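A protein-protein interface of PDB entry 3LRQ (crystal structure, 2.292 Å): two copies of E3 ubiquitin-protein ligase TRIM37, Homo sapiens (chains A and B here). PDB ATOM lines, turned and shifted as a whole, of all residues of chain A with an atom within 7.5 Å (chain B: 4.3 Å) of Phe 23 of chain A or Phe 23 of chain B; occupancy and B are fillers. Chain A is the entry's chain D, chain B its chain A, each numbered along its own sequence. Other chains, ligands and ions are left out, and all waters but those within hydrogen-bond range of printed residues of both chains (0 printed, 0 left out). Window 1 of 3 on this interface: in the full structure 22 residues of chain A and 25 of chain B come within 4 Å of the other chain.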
ATOM      1  N   GLU A  17     -15.858  -3.075  -4.678  1.00  0.00           N
ATOM      2  CA  GLU A  17     -15.782  -1.800  -5.378  1.00  0.00           C
ATOM      3  C   GLU A  17     -16.989  -1.602  -6.291  1.00  0.00           C
ATOM      4  O   GLU A  17     -17.537  -0.500  -6.376  1.00  0.00           O
ATOM      5  CB  GLU A  17     -14.477  -1.694  -6.165  1.00  0.00           C
ATOM      6  CG  GLU A  17     -14.235  -0.318  -6.749  1.00  0.00           C
ATOM      7  CD  GLU A  17     -14.381   0.788  -5.717  1.00  0.00           C
ATOM      8  OE1 GLU A  17     -14.045   0.563  -4.531  1.00  0.00           O
ATOM      9  OE2 GLU A  17     -14.833   1.889  -6.101  1.00  0.00           O
ATOM     10  N   SER A  18     -17.416  -2.672  -6.958  1.00  0.00           N
ATOM     11  CA  SER A  18     -18.661  -2.619  -7.709  1.00  0.00           C
ATOM     12  C   SER A  18     -19.787  -2.094  -6.815  1.00  0.00           C
ATOM     13  O   SER A  18     -20.522  -1.187  -7.210  1.00  0.00           O
ATOM     14  CB  SER A  18     -19.055  -3.996  -8.236  1.00  0.00           C
ATOM     15  OG  SER A  18     -18.123  -4.473  -9.179  1.00  0.00           O
ATOM     16  N   ILE A  19     -19.928  -2.665  -5.616  1.00  0.00           N
ATOM     17  CA  ILE A  19     -21.024  -2.252  -4.742  1.00  0.00           C
ATOM     18  C   ILE A  19     -20.874  -0.794  -4.331  1.00  0.00           C
ATOM     19  O   ILE A  19     -21.850  -0.052  -4.323  1.00  0.00           O
ATOM     20  CB  ILE A  19     -21.155  -3.132  -3.491  1.00  0.00           C
ATOM     21  CG1 ILE A  19     -21.525  -4.563  -3.874  1.00  0.00           C
ATOM     22  CG2 ILE A  19     -22.219  -2.567  -2.539  1.00  0.00           C
ATOM     23  CD1 ILE A  19     -21.503  -5.515  -2.689  1.00  0.00           C
ATOM     24  N   ALA A  20     -19.648  -0.395  -3.994  1.00  0.00           N
ATOM     25  CA  ALA A  20     -19.354   0.987  -3.607  1.00  0.00           C
ATOM     26  C   ALA A  20     -19.689   2.006  -4.712  1.00  0.00           C
ATOM     27  O   ALA A  20     -20.119   3.137  -4.435  1.00  0.00           O
ATOM     28  CB  ALA A  20     -17.879   1.117  -3.167  1.00  0.00           C
ATOM     29  N   GLU A  21     -19.480   1.626  -5.964  1.00  0.00           N
ATOM     30  CA  GLU A  21     -19.840   2.526  -7.071  1.00  0.00           C
ATOM     31  C   GLU A  21     -21.329   2.877  -7.020  1.00  0.00           C
ATOM     32  O   GLU A  21     -21.720   4.044  -7.155  1.00  0.00           O
ATOM     33  CB  GLU A  21     -19.486   1.908  -8.429  1.00  0.00           C
ATOM     34  CG  GLU A  21     -19.021   2.930  -9.457  1.00  0.00           C
ATOM     35  CD  GLU A  21     -17.816   3.750  -8.991  1.00  0.00           C
ATOM     36  OE1 GLU A  21     -17.193   3.391  -7.971  1.00  0.00           O
ATOM     37  OE2 GLU A  21     -17.492   4.758  -9.654  1.00  0.00           O
ATOM     38  N   VAL A  22     -22.159   1.864  -6.783  1.00  0.00           N
ATOM     39  CA  VAL A  22     -23.595   2.077  -6.703  1.00  0.00           C
ATOM     40  C   VAL A  22     -23.921   3.151  -5.671  1.00  0.00           C
ATOM     41  O   VAL A  22     -24.806   3.986  -5.885  1.00  0.00           O
ATOM     42  CB  VAL A  22     -24.335   0.760  -6.339  1.00  0.00           C
ATOM     43  CG1 VAL A  22     -25.833   1.019  -6.066  1.00  0.00           C
ATOM     44  CG2 VAL A  22     -24.141  -0.278  -7.439  1.00  0.00           C
ATOM     45  N   PHE A  23     -23.190   3.131  -4.557  1.00  0.00           N
ATOM     46  CA  PHE A  23     -23.480   4.009  -3.419  1.00  0.00           C
ATOM     47  C   PHE A  23     -22.588   5.244  -3.345  1.00  0.00           C
ATOM     48  O   PHE A  23     -22.252   5.729  -2.268  1.00  0.00           O
ATOM     49  CB  PHE A  23     -23.483   3.198  -2.104  1.00  0.00           C
ATOM     50  CG  PHE A  23     -24.576   2.188  -2.067  1.00  0.00           C
ATOM     51  CD1 PHE A  23     -25.830   2.524  -1.575  1.00  0.00           C
ATOM     52  CD2 PHE A  23     -24.389   0.933  -2.620  1.00  0.00           C
ATOM     53  CE1 PHE A  23     -26.858   1.608  -1.598  1.00  0.00           C
ATOM     54  CE2 PHE A  23     -25.416   0.005  -2.645  1.00  0.00           C
ATOM     55  CZ  PHE A  23     -26.651   0.340  -2.141  1.00  0.00           C
ATOM     56  N   ARG A  24     -22.196   5.739  -4.513  1.00  0.00           N
ATOM     57  CA  ARG A  24     -21.563   7.042  -4.601  1.00  0.00           C
ATOM     58  C   ARG A  24     -22.541   7.976  -5.272  1.00  0.00           C
ATOM     59  O   ARG A  24     -23.386   7.553  -6.044  1.00  0.00           O
ATOM     60  CB  ARG A  24     -20.221   6.981  -5.343  1.00  0.00           C
ATOM     61  CG  ARG A  24     -19.083   6.540  -4.445  1.00  0.00           C
ATOM     62  CD  ARG A  24     -17.729   6.558  -5.133  1.00  0.00           C
ATOM     63  NE  ARG A  24     -16.727   5.913  -4.286  1.00  0.00           N
ATOM     64  CZ  ARG A  24     -16.314   4.657  -4.442  1.00  0.00           C
ATOM     65  NH1 ARG A  24     -16.792   3.918  -5.436  1.00  0.00           N
ATOM     66  NH2 ARG A  24     -15.408   4.141  -3.615  1.00  0.00           N
ATOM     67  N   CYS A  25     -22.444   9.251  -4.945  1.00  0.00           N
ATOM     68  CA  CYS A  25     -23.397  10.212  -5.435  1.00  0.00           C
ATOM     69  C   CYS A  25     -23.145  10.461  -6.922  1.00  0.00           C
ATOM     70  O   CYS A  25     -22.022  10.777  -7.319  1.00  0.00           O
ATOM     71  CB  CYS A  25     -23.279  11.511  -4.638  1.00  0.00           C
ATOM     72  SG  CYS A  25     -24.175  12.890  -5.407  1.00  0.00           S
ATOM     73  N   PHE A  26     -24.180  10.320  -7.743  1.00  0.00           N
ATOM     74  CA  PHE A  26     -24.012  10.500  -9.196  1.00  0.00           C
ATOM     75  C   PHE A  26     -23.488  11.906  -9.548  1.00  0.00           C
ATOM     76  O   PHE A  26     -22.775  12.070 -10.512  1.00  0.00           O
ATOM     77  CB  PHE A  26     -25.319  10.199  -9.962  1.00  0.00           C
ATOM     78  CG  PHE A  26     -25.189  10.312 -11.459  1.00  0.00           C
ATOM     79  CD1 PHE A  26     -24.774   9.224 -12.221  1.00  0.00           C
ATOM     80  CD2 PHE A  26     -25.474  11.513 -12.109  1.00  0.00           C
ATOM     81  CE1 PHE A  26     -24.636   9.329 -13.614  1.00  0.00           C
ATOM     82  CE2 PHE A  26     -25.348  11.628 -13.495  1.00  0.00           C
ATOM     83  CZ  PHE A  26     -24.928  10.530 -14.248  1.00  0.00           C
ATOM     84  N   MET A  29     -19.892  12.572  -6.734  1.00  0.00           N
ATOM     85  CA  MET A  29     -19.046  11.376  -6.637  1.00  0.00           C
ATOM     86  C   MET A  29     -18.603  10.976  -5.224  1.00  0.00           C
ATOM     87  O   MET A  29     -17.880   9.997  -5.065  1.00  0.00           O
ATOM     88  CB  MET A  29     -17.809  11.515  -7.523  1.00  0.00           C
ATOM     89  CG  MET A  29     -18.009  12.437  -8.714  1.00  0.00           C
ATOM     90  SD  MET A  29     -17.758  11.604 -10.471  1.00  0.00           S
ATOM     91  CE  MET A  29     -19.513  10.757 -10.649  1.00  0.00           C
ATOM     92  N   GLU A  30     -19.000  11.731  -4.206  1.00  0.00           N
ATOM     93  CA  GLU A  30     -18.608  11.390  -2.840  1.00  0.00           C
ATOM     94  C   GLU A  30     -19.581  10.351  -2.265  1.00  0.00           C
ATOM     95  O   GLU A  30     -20.491   9.900  -2.964  1.00  0.00           O
ATOM     96  CB  GLU A  30     -18.531  12.643  -1.944  1.00  0.00           C
ATOM     97  CG  GLU A  30     -17.493  13.698  -2.401  1.00  0.00           C
ATOM     98  CD  GLU A  30     -16.140  13.100  -2.823  1.00  0.00           C
ATOM     99  OE1 GLU A  30     -15.600  12.230  -2.102  1.00  0.00           O
ATOM    100  OE2 GLU A  30     -15.618  13.507  -3.888  1.00  0.00           O
ATOM    101  N   LYS A  31     -19.381   9.957  -1.009  1.00  0.00           N
ATOM    102  CA  LYS A  31     -20.314   9.043  -0.364  1.00  0.00           C
ATOM    103  C   LYS A  31     -21.619   9.794  -0.186  1.00  0.00           C
ATOM    104  O   LYS A  31     -21.622  11.014  -0.102  1.00  0.00           O
ATOM    105  CB  LYS A  31     -19.782   8.531   0.983  1.00  0.00           C
ATOM    106  CG  LYS A  31     -19.678   9.576   2.093  1.00  0.00           C
ATOM    107  CD  LYS A  31     -19.365   8.909   3.447  1.00  0.00           C
ATOM    108  CE  LYS A  31     -18.133   8.004   3.359  1.00  0.00           C
ATOM    109  NZ  LYS A  31     -18.042   7.031   4.491  1.00  0.00           N
ATOM    110  N   LEU A  32     -22.734   9.083  -0.130  1.00  0.00           N
ATOM    111  CA  LEU A  32     -24.028   9.766  -0.079  1.00  0.00           C
ATOM    112  C   LEU A  32     -24.272  10.408   1.272  1.00  0.00           C
ATOM    113  O   LEU A  32     -23.928   9.836   2.305  1.00  0.00           O
ATOM    114  CB  LEU A  32     -25.150   8.788  -0.403  1.00  0.00           C
ATOM    115  CG  LEU A  32     -25.042   8.224  -1.824  1.00  0.00           C
ATOM    116  CD1 LEU A  32     -25.490   6.766  -1.836  1.00  0.00           C
ATOM    117  CD2 LEU A  32     -25.832   9.105  -2.851  1.00  0.00           C
ATOM    118  N   ARG A  33     -24.853  11.602   1.258  1.00  0.00           N
ATOM    119  CA  ARG A  33     -25.328  12.237   2.477  1.00  0.00           C
ATOM    120  C   ARG A  33     -26.806  12.465   2.314  1.00  0.00           C
ATOM    121  O   ARG A  33     -27.211  13.156   1.390  1.00  0.00           O
ATOM    122  CB  ARG A  33     -24.626  13.573   2.698  1.00  0.00           C
ATOM    123  CG  ARG A  33     -23.111  13.461   2.675  1.00  0.00           C
ATOM    124  CD  ARG A  33     -22.440  14.818   2.509  1.00  0.00           C
ATOM    125  NE  ARG A  33     -22.501  15.351   1.145  1.00  0.00           N
ATOM    126  CZ  ARG A  33     -23.364  16.277   0.738  1.00  0.00           C
ATOM    127  NH1 ARG A  33     -24.262  16.772   1.584  1.00  0.00           N
ATOM    128  NH2 ARG A  33     -23.334  16.708  -0.519  1.00  0.00           N
ATOM    129  N   ALA A  35     -29.029  10.287   1.304  1.00  0.00           N
ATOM    130  CA  ALA A  35     -29.224   9.738  -0.030  1.00  0.00           C
ATOM    131  C   ALA A  35     -30.657   9.858  -0.522  1.00  0.00           C
ATOM    132  O   ALA A  35     -31.599   9.528   0.200  1.00  0.00           O
ATOM    133  CB  ALA A  35     -28.804   8.284  -0.045  1.00  0.00           C
ATOM    134  N   LEU A  44     -28.676   7.102  -7.299  1.00  0.00           N
ATOM    135  CA  LEU A  44     -28.652   7.772  -5.982  1.00  0.00           C
ATOM    136  C   LEU A  44     -27.808   9.052  -5.970  1.00  0.00           C
ATOM    137  O   LEU A  44     -26.711   9.098  -6.554  1.00  0.00           O
ATOM    138  CB  LEU A  44     -28.103   6.812  -4.923  1.00  0.00           C
ATOM    139  CG  LEU A  44     -28.863   5.498  -4.699  1.00  0.00           C
ATOM    140  CD1 LEU A  44     -27.953   4.423  -4.161  1.00  0.00           C
ATOM    141  CD2 LEU A  44     -29.978   5.746  -3.723  1.00  0.00           C
ATOM    142  N   CYS A  76     -33.801   7.368   0.705  1.00  0.00           N
ATOM    143  CA  CYS A  76     -33.274   6.031   0.934  1.00  0.00           C
ATOM    144  C   CYS A  76     -32.803   5.887   2.384  1.00  0.00           C
ATOM    145  O   CYS A  76     -31.672   6.213   2.725  1.00  0.00           O
ATOM    146  CB  CYS A  76     -32.152   5.706  -0.060  1.00  0.00           C
ATOM    147  SG  CYS A  76     -32.763   5.556  -1.755  1.00  0.00           S
ATOM    148  N   TRP A  78     -32.143   3.378   4.296  1.00  0.00           N
ATOM    149  CA  TRP A  78     -31.141   2.367   4.588  1.00  0.00           C
ATOM    150  C   TRP A  78     -29.776   2.747   4.011  1.00  0.00           C
ATOM    151  O   TRP A  78     -28.799   2.029   4.205  1.00  0.00           O
ATOM    152  CB  TRP A  78     -31.595   1.017   4.015  1.00  0.00           C
ATOM    153  CG  TRP A  78     -32.250   1.178   2.698  1.00  0.00           C
ATOM    154  CD1 TRP A  78     -33.593   1.182   2.443  1.00  0.00           C
ATOM    155  CD2 TRP A  78     -31.602   1.408   1.444  1.00  0.00           C
ATOM    156  NE1 TRP A  78     -33.819   1.379   1.103  1.00  0.00           N
ATOM    157  CE2 TRP A  78     -32.617   1.521   0.463  1.00  0.00           C
ATOM    158  CE3 TRP A  78     -30.268   1.506   1.045  1.00  0.00           C
ATOM    159  CZ2 TRP A  78     -32.332   1.748  -0.896  1.00  0.00           C
ATOM    160  CZ3 TRP A  78     -29.985   1.730  -0.306  1.00  0.00           C
ATOM    161  CH2 TRP A  78     -31.017   1.850  -1.256  1.00  0.00           C
ATOM    162  N   ALA A  79     -29.699   3.859   3.286  1.00  0.00           N
ATOM    163  CA  ALA A  79     -28.458   4.160   2.583  1.00  0.00           C
ATOM    164  C   ALA A  79     -27.296   4.413   3.535  1.00  0.00           C
ATOM    165  O   ALA A  79     -26.171   3.994   3.263  1.00  0.00           O
ATOM    166  CB  ALA A  79     -28.629   5.336   1.618  1.00  0.00           C
ATOM    167  N   GLU A  80     -27.558   5.111   4.635  1.00  0.00           N
ATOM    168  CA  GLU A  80     -26.494   5.459   5.575  1.00  0.00           C
ATOM    169  C   GLU A  80     -25.886   4.197   6.160  1.00  0.00           C
ATOM    170  O   GLU A  80     -24.667   4.026   6.178  1.00  0.00           O
ATOM    171  CB  GLU A  80     -27.028   6.350   6.696  1.00  0.00           C
ATOM    172  CG  GLU A  80     -25.932   6.887   7.643  1.00  0.00           C
ATOM    173  CD  GLU A  80     -26.492   7.802   8.749  1.00  0.00           C
ATOM    174  OE1 GLU A  80     -27.617   8.326   8.585  1.00  0.00           O
ATOM    175  OE2 GLU A  80     -25.808   7.997   9.783  1.00  0.00           O
ATOM    176  N   VAL A  82     -25.793   1.232   4.880  1.00  0.00           N
ATOM    177  CA  VAL A  82     -24.981   0.574   3.865  1.00  0.00           C
ATOM    178  C   VAL A  82     -23.668   1.328   3.679  1.00  0.00           C
ATOM    179  O   VAL A  82     -22.603   0.723   3.579  1.00  0.00           O
ATOM    180  CB  VAL A  82     -25.736   0.458   2.509  1.00  0.00           C
ATOM    181  CG1 VAL A  82     -24.801  -0.047   1.417  1.00  0.00           C
ATOM    182  CG2 VAL A  82     -26.955  -0.463   2.640  1.00  0.00           C
ATOM    183  N   THR A  83     -23.745   2.655   3.639  1.00  0.00           N
ATOM    184  CA  THR A  83     -22.546   3.477   3.465  1.00  0.00           C
ATOM    185  C   THR A  83     -21.553   3.142   4.586  1.00  0.00           C
ATOM    186  O   THR A  83     -20.364   2.929   4.342  1.00  0.00           O
ATOM    187  CB  THR A  83     -22.876   4.999   3.506  1.00  0.00           C
ATOM    188  OG1 THR A  83     -23.672   5.365   2.372  1.00  0.00           O
ATOM    189  CG2 THR A  83     -21.608   5.829   3.513  1.00  0.00           C
ATOM    190  N   LEU A  86     -19.983  -0.371   4.059  1.00  0.00           N
ATOM    191  CA  LEU A  86     -19.034  -0.238   2.954  1.00  0.00           C
ATOM    192  C   LEU A  86     -17.704   0.319   3.445  1.00  0.00           C
ATOM    193  O   LEU A  86     -16.637  -0.163   3.083  1.00  0.00           O
ATOM    194  CB  LEU A  86     -19.602   0.707   1.899  1.00  0.00           C
ATOM    195  CG  LEU A  86     -19.957   0.152   0.520  1.00  0.00           C
ATOM    196  CD1 LEU A  86     -19.985  -1.362   0.485  1.00  0.00           C
ATOM    197  CD2 LEU A  86     -21.283   0.734   0.034  1.00  0.00           C
ATOM    198  N   ILE B  19     -24.947  -5.670   5.039  1.00  0.00           N
ATOM    199  CA  ILE B  19     -25.432  -5.179   3.752  1.00  0.00           C
ATOM    200  C   ILE B  19     -26.473  -6.124   3.164  1.00  0.00           C
ATOM    201  O   ILE B  19     -27.529  -5.686   2.710  1.00  0.00           O
ATOM    202  CB  ILE B  19     -24.283  -4.937   2.734  1.00  0.00           C
ATOM    203  CG1 ILE B  19     -23.344  -3.853   3.251  1.00  0.00           C
ATOM    204  CG2 ILE B  19     -24.830  -4.475   1.370  1.00  0.00           C
ATOM    205  CD1 ILE B  19     -22.176  -3.590   2.342  1.00  0.00           C
ATOM    206  N   ALA B  20     -26.191  -7.422   3.182  1.00  0.00           N
ATOM    207  CA  ALA B  20     -27.126  -8.370   2.587  1.00  0.00           C
ATOM    208  C   ALA B  20     -28.486  -8.266   3.260  1.00  0.00           C
ATOM    209  O   ALA B  20     -29.525  -8.414   2.604  1.00  0.00           O
ATOM    210  CB  ALA B  20     -26.595  -9.789   2.663  1.00  0.00           C
ATOM    211  N   GLU B  21     -28.479  -7.988   4.564  1.00  0.00           N
ATOM    212  CA  GLU B  21     -29.719  -7.926   5.319  1.00  0.00           C
ATOM    213  C   GLU B  21     -30.551  -6.764   4.801  1.00  0.00           C
ATOM    214  O   GLU B  21     -31.766  -6.870   4.688  1.00  0.00           O
ATOM    215  CB  GLU B  21     -29.466  -7.825   6.843  1.00  0.00           C
ATOM    216  CG  GLU B  21     -30.693  -8.157   7.731  1.00  0.00           C
ATOM    217  CD  GLU B  21     -31.250  -9.578   7.523  1.00  0.00           C
ATOM    218  OE1 GLU B  21     -30.520 -10.440   6.982  1.00  0.00           O
ATOM    219  OE2 GLU B  21     -32.423  -9.833   7.902  1.00  0.00           O
ATOM    220  N   VAL B  22     -29.896  -5.663   4.452  1.00  0.00           N
ATOM    221  CA  VAL B  22     -30.632  -4.533   3.888  1.00  0.00           C
ATOM    222  C   VAL B  22     -31.328  -4.914   2.568  1.00  0.00           C
ATOM    223  O   VAL B  22     -32.410  -4.422   2.255  1.00  0.00           O
ATOM    224  CB  VAL B  22     -29.698  -3.334   3.617  1.00  0.00           C
ATOM    225  CG1 VAL B  22     -30.433  -2.265   2.788  1.00  0.00           C
ATOM    226  CG2 VAL B  22     -29.133  -2.768   4.935  1.00  0.00           C
ATOM    227  N   PHE B  23     -30.695  -5.788   1.790  1.00  0.00           N
ATOM    228  CA  PHE B  23     -31.226  -6.146   0.489  1.00  0.00           C
ATOM    229  C   PHE B  23     -31.951  -7.488   0.496  1.00  0.00           C
ATOM    230  O   PHE B  23     -31.755  -8.347  -0.372  1.00  0.00           O
ATOM    231  CB  PHE B  23     -30.128  -6.056  -0.566  1.00  0.00           C
ATOM    232  CG  PHE B  23     -29.562  -4.679  -0.683  1.00  0.00           C
ATOM    233  CD1 PHE B  23     -30.306  -3.671  -1.260  1.00  0.00           C
ATOM    234  CD2 PHE B  23     -28.326  -4.374  -0.167  1.00  0.00           C
ATOM    235  CE1 PHE B  23     -29.811  -2.399  -1.349  1.00  0.00           C
ATOM    236  CE2 PHE B  23     -27.832  -3.105  -0.250  1.00  0.00           C
ATOM    237  CZ  PHE B  23     -28.577  -2.116  -0.851  1.00  0.00           C
ATOM    238  N   ARG B  24     -32.806  -7.634   1.498  1.00  0.00           N
ATOM    239  CA  ARG B  24     -33.702  -8.763   1.609  1.00  0.00           C
ATOM    240  C   ARG B  24     -35.120  -8.220   1.508  1.00  0.00           C
ATOM    241  O   ARG B  24     -35.384  -7.066   1.846  1.00  0.00           O
ATOM    242  CB  ARG B  24     -33.467  -9.510   2.916  1.00  0.00           C
ATOM    243  CG  ARG B  24     -32.270 -10.463   2.858  1.00  0.00           C
ATOM    244  CD  ARG B  24     -32.114 -11.284   4.140  1.00  0.00           C
ATOM    245  NE  ARG B  24     -31.147 -12.380   4.001  1.00  0.00           N
ATOM    246  CZ  ARG B  24     -29.849 -12.296   4.304  1.00  0.00           C
ATOM    247  NH1 ARG B  24     -29.331 -11.160   4.750  1.00  0.00           N
ATOM    248  NH2 ARG B  24     -29.057 -13.351   4.154  1.00  0.00           N
ATOM    249  N   LYS B  31     -33.532 -13.170  -0.361  1.00  0.00           N
ATOM    250  CA  LYS B  31     -32.777 -12.190  -1.115  1.00  0.00           C
ATOM    251  C   LYS B  31     -33.664 -11.724  -2.265  1.00  0.00           C
ATOM    252  O   LYS B  31     -34.510 -12.463  -2.756  1.00  0.00           O
ATOM    253  CB  LYS B  31     -31.406 -12.706  -1.566  1.00  0.00           C
ATOM    254  CG  LYS B  31     -31.418 -13.704  -2.692  1.00  0.00           C
ATOM    255  CD  LYS B  31     -30.310 -13.378  -3.694  1.00  0.00           C
ATOM    256  CE  LYS B  31     -29.853 -14.607  -4.477  1.00  0.00           C
ATOM    257  NZ  LYS B  31     -28.990 -15.494  -3.638  1.00  0.00           N
ATOM    258  N   LEU B  32     -33.495 -10.476  -2.659  1.00  0.00           N
ATOM    259  CA  LEU B  32     -34.436  -9.833  -3.550  1.00  0.00           C
ATOM    260  C   LEU B  32     -34.367 -10.428  -4.950  1.00  0.00           C
ATOM    261  O   LEU B  32     -33.278 -10.627  -5.486  1.00  0.00           O
ATOM    262  CB  LEU B  32     -34.161  -8.324  -3.599  1.00  0.00           C
ATOM    263  CG  LEU B  32     -34.592  -7.501  -2.379  1.00  0.00           C
ATOM    264  CD1 LEU B  32     -33.769  -6.215  -2.282  1.00  0.00           C
ATOM    265  CD2 LEU B  32     -36.074  -7.184  -2.452  1.00  0.00           C
ATOM    266  N   LEU B  44     -37.681  -2.356   0.366  1.00  0.00           N
ATOM    267  CA  LEU B  44     -37.568  -3.145  -0.856  1.00  0.00           C
ATOM    268  C   LEU B  44     -38.318  -4.475  -0.728  1.00  0.00           C
ATOM    269  O   LEU B  44     -38.263  -5.109   0.326  1.00  0.00           O
ATOM    270  CB  LEU B  44     -36.084  -3.420  -1.161  1.00  0.00           C
ATOM    271  CG  LEU B  44     -35.171  -2.239  -1.533  1.00  0.00           C
ATOM    272  CD1 LEU B  44     -33.913  -2.234  -0.691  1.00  0.00           C
ATOM    273  CD2 LEU B  44     -34.803  -2.214  -3.033  1.00  0.00           C
ATOM    274  N   TRP B  78     -30.227  -1.309  -9.929  1.00  0.00           N
ATOM    275  CA  TRP B  78     -28.917  -1.826  -9.559  1.00  0.00           C
ATOM    276  C   TRP B  78     -29.025  -2.978  -8.560  1.00  0.00           C
ATOM    277  O   TRP B  78     -28.035  -3.636  -8.234  1.00  0.00           O
ATOM    278  CB  TRP B  78     -28.085  -0.695  -8.969  1.00  0.00           C
ATOM    279  CG  TRP B  78     -28.858   0.203  -8.066  1.00  0.00           C
ATOM    280  CD1 TRP B  78     -29.371   1.441  -8.372  1.00  0.00           C
ATOM    281  CD2 TRP B  78     -29.248  -0.070  -6.705  1.00  0.00           C
ATOM    282  NE1 TRP B  78     -30.040   1.959  -7.280  1.00  0.00           N
ATOM    283  CE2 TRP B  78     -29.976   1.055  -6.245  1.00  0.00           C
ATOM    284  CE3 TRP B  78     -29.031  -1.139  -5.828  1.00  0.00           C
ATOM    285  CZ2 TRP B  78     -30.483   1.140  -4.944  1.00  0.00           C
ATOM    286  CZ3 TRP B  78     -29.548  -1.059  -4.529  1.00  0.00           C
ATOM    287  CH2 TRP B  78     -30.269   0.070  -4.106  1.00  0.00           C
ATOM    288  N   VAL B  82     -25.920  -5.590  -7.166  1.00  0.00           N
ATOM    289  CA  VAL B  82     -25.496  -5.577  -5.770  1.00  0.00           C
ATOM    290  C   VAL B  82     -25.711  -6.945  -5.121  1.00  0.00           C
ATOM    291  O   VAL B  82     -24.843  -7.486  -4.438  1.00  0.00           O
ATOM    292  CB  VAL B  82     -26.244  -4.519  -4.991  1.00  0.00           C
ATOM    293  CG1 VAL B  82     -26.040  -4.715  -3.471  1.00  0.00           C
ATOM    294  CG2 VAL B  82     -25.788  -3.154  -5.465  1.00  0.00           C
ATOM    295  N   LEU B  86     -22.946  -9.442  -3.619  1.00  0.00           N
ATOM    296  CA  LEU B  86     -23.032  -9.895  -2.225  1.00  0.00           C
ATOM    297  C   LEU B  86     -22.920 -11.407  -2.147  1.00  0.00           C
ATOM    298  O   LEU B  86     -22.317 -11.945  -1.219  1.00  0.00           O
ATOM    299  CB  LEU B  86     -24.330  -9.447  -1.554  1.00  0.00           C
ATOM    300  CG  LEU B  86     -24.416  -7.966  -1.196  1.00  0.00           C
ATOM    301  CD1 LEU B  86     -25.840  -7.613  -0.753  1.00  0.00           C
ATOM    302  CD2 LEU B  86     -23.397  -7.608  -0.118  1.00  0.00           C
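Among the printed residues, merely in contact across the chains: Phe 23 of chain A with Phe 23 of chain B (3.4 Å), Trp 78 of chain A with Trp 78 of chain B (3.4 Å), Leu 86 of chain A with Ile 19 of chain B (3.6 Å), Val 22 of chain A with Trp 78 of chain B (3.6 Å), Trp 78 of chain A with Val 22 of chain B (3.7 Å), Ile 19 of chain A with Leu 86 of chain B (3.8 Å), Val 22 of chain A with Val 82 of chain B (3.9 Å) and Val 82 of chain A with Val 22 of chain B (3.9 Å).
Of the printed residues of chain B, Val 22 of chain A touches Trp 78 (3.6 Å) and Val 82 (3.9 Å). Of the printed residues of chain B, Phe 23 of chain A touches Phe 23 (3.4 Å). Leu 44 of chain A touches none of the printed residues of chain B. Printed residues of chain B within 4 Å of Val 82 of chain A: Val 22 (3.9 Å). Of the printed residues of chain B, Leu 86 of chain A touches Ile 19 (3.6 Å). Printed residues of chain A within 4 Å of Val 22 of chain B: Trp 78 (3.7 Å) and Val 82 (3.9 Å). Of the printed residues of chain A, Phe 23 of chain B touches Phe 23 (3.4 Å). Of the printed residues of chain A, Val 82 of chain B touches Val 22. The nearest printed residue of chain B that does not touch Phe 23 of chain A is Trp 78 of chain B (4.01 Å). The nearest printed residue of chain A that does not touch Leu 86 of chain B is Leu 86 of chain A (7.1 Å).
Of the 12 printed residues of chain B, 6 touch a printed residue of chain A. Hydrophobic or aromatic side chains of chain B that line the printed part of chain A: Ile 19, Val 22, Phe 23, Trp 78, Val 82 and Leu 86. Of the 24 printed residues of chain A, 6 touch a printed residue of chain B. Hydrophobic or aromatic side chains of chain A that line the printed part of chain B: Ile 19, Val 22, Phe 23, Trp 78, Val 82 and Leu 86. Among the printed residues, no Asp or Glu carboxylate lies within 4 Å of a Lys or Arg side-chain nitrogen of the other chain.
Val 22 of chain A touches Trp 78 of chain B, and with the chains exchanged Trp 78 of chain A touches Val 22 of chain B. Val 22 of chain A touches Val 82 of chain B, and with the chains exchanged Val 82 of chain A touches Val 22 of chain B. Phe 23 of chain A touches its own counterpart, Phe 23 of chain B. Trp 78 of chain A touches its own counterpart, Trp 78 of chain B. Positions printed for both chains: 19, 20, 21, 22, 23, 24, 31, 32, 44, 78, 82 and 86.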
